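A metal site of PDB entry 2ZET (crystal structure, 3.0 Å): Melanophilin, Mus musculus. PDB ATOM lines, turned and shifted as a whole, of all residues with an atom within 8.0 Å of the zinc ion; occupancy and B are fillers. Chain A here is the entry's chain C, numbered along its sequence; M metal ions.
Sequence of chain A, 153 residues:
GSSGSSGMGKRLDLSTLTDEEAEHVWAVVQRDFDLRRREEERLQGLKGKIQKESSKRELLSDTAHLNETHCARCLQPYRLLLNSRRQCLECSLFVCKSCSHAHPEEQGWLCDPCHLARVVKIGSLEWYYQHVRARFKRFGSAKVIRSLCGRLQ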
ATOM      1  N   HIS A  70       6.841 -11.680  15.326  1.00  0.00           N
ATOM      2  CA  HIS A  70       5.781 -12.401  14.630  1.00  0.00           C
ATOM      3  C   HIS A  70       5.787 -13.910  14.900  1.00  0.00           C
ATOM      4  O   HIS A  70       6.856 -14.514  15.004  1.00  0.00           O
ATOM      5  CB  HIS A  70       5.928 -12.140  13.136  1.00  0.00           C
ATOM      6  CG  HIS A  70       5.800 -10.700  12.756  1.00  0.00           C
ATOM      7  ND1 HIS A  70       4.649 -10.167  12.213  1.00  0.00           N
ATOM      8  CD2 HIS A  70       6.681  -9.673  12.868  1.00  0.00           C
ATOM      9  CE1 HIS A  70       4.819  -8.878  12.015  1.00  0.00           C
ATOM     10  NE2 HIS A  70       6.037  -8.549  12.400  1.00  0.00           N
ATOM     11  N   CYS A  71       4.607 -14.507  15.007  1.00  0.00           N
ATOM     12  CA  CYS A  71       4.508 -15.963  15.213  1.00  0.00           C
ATOM     13  C   CYS A  71       5.216 -16.670  14.058  1.00  0.00           C
ATOM     14  O   CYS A  71       5.035 -16.311  12.883  1.00  0.00           O
ATOM     15  CB  CYS A  71       3.043 -16.430  15.250  1.00  0.00           C
ATOM     16  SG  CYS A  71       2.866 -18.236  15.295  1.00  0.00           S
ATOM     17  N   ALA A  72       6.015 -17.681  14.391  1.00  0.00           N
ATOM     18  CA  ALA A  72       6.775 -18.442  13.397  1.00  0.00           C
ATOM     19  C   ALA A  72       5.903 -19.239  12.422  1.00  0.00           C
ATOM     20  O   ALA A  72       6.357 -19.612  11.342  1.00  0.00           O
ATOM     21  CB  ALA A  72       7.750 -19.386  14.113  1.00  0.00           C
ATOM     22  N   ARG A  73       4.646 -19.464  12.793  1.00  0.00           N
ATOM     23  CA  ARG A  73       3.745 -20.239  11.969  1.00  0.00           C
ATOM     24  C   ARG A  73       2.772 -19.384  11.166  1.00  0.00           C
ATOM     25  O   ARG A  73       2.780 -19.426   9.949  1.00  0.00           O
ATOM     26  CB  ARG A  73       2.972 -21.210  12.858  1.00  0.00           C
ATOM     27  CG  ARG A  73       2.549 -22.508  12.210  1.00  0.00           C
ATOM     28  CD  ARG A  73       1.670 -22.288  11.011  1.00  0.00           C
ATOM     29  NE  ARG A  73       0.741 -23.384  10.828  1.00  0.00           N
ATOM     30  CZ  ARG A  73      -0.044 -23.528   9.772  1.00  0.00           C
ATOM     31  NH1 ARG A  73      -0.007 -22.631   8.777  1.00  0.00           N
ATOM     32  NH2 ARG A  73      -0.875 -24.571   9.714  1.00  0.00           N
ATOM     33  N   CYS A  74       1.922 -18.600  11.842  1.00  0.00           N
ATOM     34  CA  CYS A  74       0.956 -17.769  11.138  1.00  0.00           C
ATOM     35  C   CYS A  74       1.457 -16.365  10.800  1.00  0.00           C
ATOM     36  O   CYS A  74       0.795 -15.625  10.074  1.00  0.00           O
ATOM     37  CB  CYS A  74      -0.358 -17.676  11.939  1.00  0.00           C
ATOM     38  SG  CYS A  74      -0.358 -16.733  13.511  1.00  0.00           S
ATOM     39  N   LEU A  75       2.626 -16.003  11.302  1.00  0.00           N
ATOM     40  CA  LEU A  75       3.226 -14.707  11.021  1.00  0.00           C
ATOM     41  C   LEU A  75       2.443 -13.511  11.533  1.00  0.00           C
ATOM     42  O   LEU A  75       2.867 -12.375  11.354  1.00  0.00           O
ATOM     43  CB  LEU A  75       3.429 -14.545   9.523  1.00  0.00           C
ATOM     44  CG  LEU A  75       4.266 -15.633   8.852  1.00  0.00           C
ATOM     45  CD1 LEU A  75       4.420 -15.278   7.376  1.00  0.00           C
ATOM     46  CD2 LEU A  75       5.631 -15.773   9.507  1.00  0.00           C
ATOM     47  N   GLN A  76       1.316 -13.747  12.169  1.00  0.00           N
ATOM     48  CA  GLN A  76       0.538 -12.640  12.711  1.00  0.00           C
ATOM     49  C   GLN A  76       1.385 -11.978  13.784  1.00  0.00           C
ATOM     50  O   GLN A  76       2.300 -12.601  14.323  1.00  0.00           O
ATOM     51  CB  GLN A  76      -0.765 -13.170  13.318  1.00  0.00           C
ATOM     52  CG  GLN A  76      -1.864 -13.357  12.294  1.00  0.00           C
ATOM     53  CD  GLN A  76      -2.611 -12.075  12.004  1.00  0.00           C
ATOM     54  OE1 GLN A  76      -3.643 -11.802  12.604  1.00  0.00           O
ATOM     55  NE2 GLN A  76      -2.069 -11.261  11.104  1.00  0.00           N
ATOM     56  N   PRO A  77       1.122 -10.688  14.100  1.00  0.00           N
ATOM     57  CA  PRO A  77       1.904  -9.996  15.137  1.00  0.00           C
ATOM     58  C   PRO A  77       1.423 -10.343  16.565  1.00  0.00           C
ATOM     59  O   PRO A  77       0.232 -10.356  16.853  1.00  0.00           O
ATOM     60  CB  PRO A  77       1.671  -8.511  14.807  1.00  0.00           C
ATOM     61  CG  PRO A  77       1.201  -8.511  13.400  1.00  0.00           C
ATOM     62  CD  PRO A  77       0.352  -9.728  13.304  1.00  0.00           C
ATOM     63  N   TYR A  78       2.353 -10.608  17.466  1.00  0.00           N
ATOM     64  CA  TYR A  78       2.024 -10.947  18.840  1.00  0.00           C
ATOM     65  C   TYR A  78       1.060  -9.996  19.559  1.00  0.00           C
ATOM     66  O   TYR A  78       0.031 -10.417  20.068  1.00  0.00           O
ATOM     67  CB  TYR A  78       3.297 -11.062  19.657  1.00  0.00           C
ATOM     68  CG  TYR A  78       4.179 -12.194  19.251  1.00  0.00           C
ATOM     69  CD1 TYR A  78       5.548 -12.059  19.249  1.00  0.00           C
ATOM     70  CD2 TYR A  78       3.634 -13.423  18.879  1.00  0.00           C
ATOM     71  CE1 TYR A  78       6.377 -13.107  18.874  1.00  0.00           C
ATOM     72  CE2 TYR A  78       4.448 -14.486  18.491  1.00  0.00           C
ATOM     73  CZ  TYR A  78       5.817 -14.320  18.496  1.00  0.00           C
ATOM     74  OH  TYR A  78       6.640 -15.327  18.073  1.00  0.00           O
ATOM     75  N   LEU A  81      -2.774 -10.506  19.314  1.00  0.00           N
ATOM     76  CA  LEU A  81      -3.461 -11.713  19.784  1.00  0.00           C
ATOM     77  C   LEU A  81      -4.071 -11.647  21.175  1.00  0.00           C
ATOM     78  O   LEU A  81      -3.786 -10.714  21.925  1.00  0.00           O
ATOM     79  CB  LEU A  81      -2.480 -12.880  19.736  1.00  0.00           C
ATOM     80  CG  LEU A  81      -1.814 -13.017  18.372  1.00  0.00           C
ATOM     81  CD1 LEU A  81      -0.693 -14.009  18.428  1.00  0.00           C
ATOM     82  CD2 LEU A  81      -2.845 -13.429  17.358  1.00  0.00           C
ATOM     83  N   ASN A  83      -3.999 -14.527  23.170  1.00  0.00           N
ATOM     84  CA  ASN A  83      -3.343 -15.570  23.938  1.00  0.00           C
ATOM     85  C   ASN A  83      -1.928 -15.081  24.197  1.00  0.00           C
ATOM     86  O   ASN A  83      -1.647 -13.899  24.036  1.00  0.00           O
ATOM     87  CB  ASN A  83      -3.341 -16.874  23.150  1.00  0.00           C
ATOM     88  CG  ASN A  83      -2.978 -16.665  21.670  1.00  0.00           C
ATOM     89  OD1 ASN A  83      -3.854 -16.351  20.851  1.00  0.00           O
ATOM     90  ND2 ASN A  83      -1.696 -16.847  21.333  1.00  0.00           N
ATOM     91  N   PHE A  94       9.302 -19.159  18.550  1.00  0.00           N
ATOM     92  CA  PHE A  94       8.066 -18.821  19.231  1.00  0.00           C
ATOM     93  C   PHE A  94       6.895 -18.846  18.288  1.00  0.00           C
ATOM     94  O   PHE A  94       7.033 -18.574  17.100  1.00  0.00           O
ATOM     95  CB  PHE A  94       8.154 -17.450  19.879  1.00  0.00           C
ATOM     96  CG  PHE A  94       9.268 -17.318  20.872  1.00  0.00           C
ATOM     97  CD1 PHE A  94      10.602 -17.292  20.444  1.00  0.00           C
ATOM     98  CD2 PHE A  94       8.991 -17.208  22.222  1.00  0.00           C
ATOM     99  CE1 PHE A  94      11.639 -17.156  21.350  1.00  0.00           C
ATOM    100  CE2 PHE A  94      10.029 -17.074  23.152  1.00  0.00           C
ATOM    101  CZ  PHE A  94      11.357 -17.052  22.712  1.00  0.00           C
ATOM    102  N   VAL A  95       5.727 -19.166  18.838  1.00  0.00           N
ATOM    103  CA  VAL A  95       4.503 -19.228  18.075  1.00  0.00           C
ATOM    104  C   VAL A  95       3.340 -18.902  18.997  1.00  0.00           C
ATOM    105  O   VAL A  95       3.466 -18.990  20.224  1.00  0.00           O
ATOM    106  CB  VAL A  95       4.284 -20.622  17.499  1.00  0.00           C
ATOM    107  CG1 VAL A  95       5.478 -21.028  16.665  1.00  0.00           C
ATOM    108  CG2 VAL A  95       4.094 -21.612  18.613  1.00  0.00           C
ATOM    109  N   CYS A  96       2.206 -18.518  18.425  1.00  0.00           N
ATOM    110  CA  CYS A  96       1.039 -18.179  19.227  1.00  0.00           C
ATOM    111  C   CYS A  96       0.380 -19.440  19.763  1.00  0.00           C
ATOM    112  O   CYS A  96       0.719 -20.546  19.353  1.00  0.00           O
ATOM    113  CB  CYS A  96       0.030 -17.357  18.409  1.00  0.00           C
ATOM    114  SG  CYS A  96      -0.992 -18.202  17.155  1.00  0.00           S
ATOM    115  N   LYS A  97      -0.545 -19.250  20.699  1.00  0.00           N
ATOM    116  CA  LYS A  97      -1.265 -20.369  21.286  1.00  0.00           C
ATOM    117  C   LYS A  97      -1.923 -21.218  20.207  1.00  0.00           C
ATOM    118  O   LYS A  97      -1.817 -22.447  20.208  1.00  0.00           O
ATOM    119  CB  LYS A  97      -2.343 -19.846  22.251  1.00  0.00           C
ATOM    120  CG  LYS A  97      -3.203 -20.927  22.930  1.00  0.00           C
ATOM    121  CD  LYS A  97      -4.329 -20.339  23.793  1.00  0.00           C
ATOM    122  CE  LYS A  97      -5.295 -21.426  24.250  1.00  0.00           C
ATOM    123  NZ  LYS A  97      -6.428 -20.878  25.064  1.00  0.00           N
ATOM    124  N   SER A  98      -2.596 -20.556  19.277  1.00  0.00           N
ATOM    125  CA  SER A  98      -3.294 -21.251  18.203  1.00  0.00           C
ATOM    126  C   SER A  98      -2.412 -22.138  17.335  1.00  0.00           C
ATOM    127  O   SER A  98      -2.887 -23.110  16.761  1.00  0.00           O
ATOM    128  CB  SER A  98      -3.992 -20.217  17.322  1.00  0.00           C
ATOM    129  OG  SER A  98      -4.520 -19.163  18.112  1.00  0.00           O
ATOM    130  N   CYS A  99      -1.133 -21.811  17.245  1.00  0.00           N
ATOM    131  CA  CYS A  99      -0.203 -22.576  16.416  1.00  0.00           C
ATOM    132  C   CYS A  99       0.698 -23.480  17.242  1.00  0.00           C
ATOM    133  O   CYS A  99       1.626 -24.091  16.729  1.00  0.00           O
ATOM    134  CB  CYS A  99       0.657 -21.619  15.588  1.00  0.00           C
ATOM    135  SG  CYS A  99      -0.282 -20.486  14.538  1.00  0.00           S
ATOM    136  N   SER A 100       0.397 -23.578  18.533  1.00  0.00           N
ATOM    137  CA  SER A 100       1.186 -24.390  19.431  1.00  0.00           C
ATOM    138  C   SER A 100       0.381 -25.579  19.940  1.00  0.00           C
ATOM    139  O   SER A 100      -0.837 -25.608  19.820  1.00  0.00           O
ATOM    140  CB  SER A 100       1.641 -23.550  20.620  1.00  0.00           C
ATOM    141  OG  SER A 100       0.553 -22.871  21.216  1.00  0.00           O
ATOM    142  N   ASP A 112       2.971 -26.086  15.844  1.00  0.00           N
ATOM    143  CA  ASP A 112       2.154 -26.903  14.930  1.00  0.00           C
ATOM    144  C   ASP A 112       2.936 -27.736  13.915  1.00  0.00           C
ATOM    145  O   ASP A 112       2.482 -28.792  13.500  1.00  0.00           O
ATOM    146  CB  ASP A 112       1.088 -26.049  14.233  1.00  0.00           C
ATOM    147  CG  ASP A 112      -0.293 -26.223  14.869  1.00  0.00           C
ATOM    148  OD1 ASP A 112      -0.727 -27.385  14.996  1.00  0.00           O
ATOM    149  OD2 ASP A 112      -0.943 -25.220  15.256  1.00  0.00           O
HETATM  150 ZN    ZN M   1       0.495 -18.220  15.094  1.00  0.00          ZN
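The backbone NH (N) of Cys 71 lies within hydrogen-bond range of the backbone carbonyl oxygen (O) of Gln 76 (3.1 Å). O of Cys 96 lies within hydrogen-bond range of OG of Ser 100 (3.0 Å). O of Cys 99 is in hydrogen-bond range of N of Asp 112 (2.6 Å). The backbone NH (N) of Arg 73 sits close to the side-chain sulfur (SG) of Cys 71, at 3.3 Å. The side-chain sulfur (SG) of Cys 96 lies close to the backbone NH (N) of Ser 98. N of Gln 76 lies close to SG of Cys 74 (3.7 Å).
Within 4 Å of the zinc ion: Cys 71, Cys 74, Cys 96 and Cys 99.
SG of Cys 74 is bound to the zinc ion, at 2.3 Å. SG of Cys 71 is bound to the zinc ion, at 2.4 Å. SG of Cys 99 is bound to the zinc ion (2.5 Å). The zinc ion is bound by the side-chain sulfur (SG) of Cys 96 (2.5 Å). The zinc ion has four donor atoms within binding distance.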
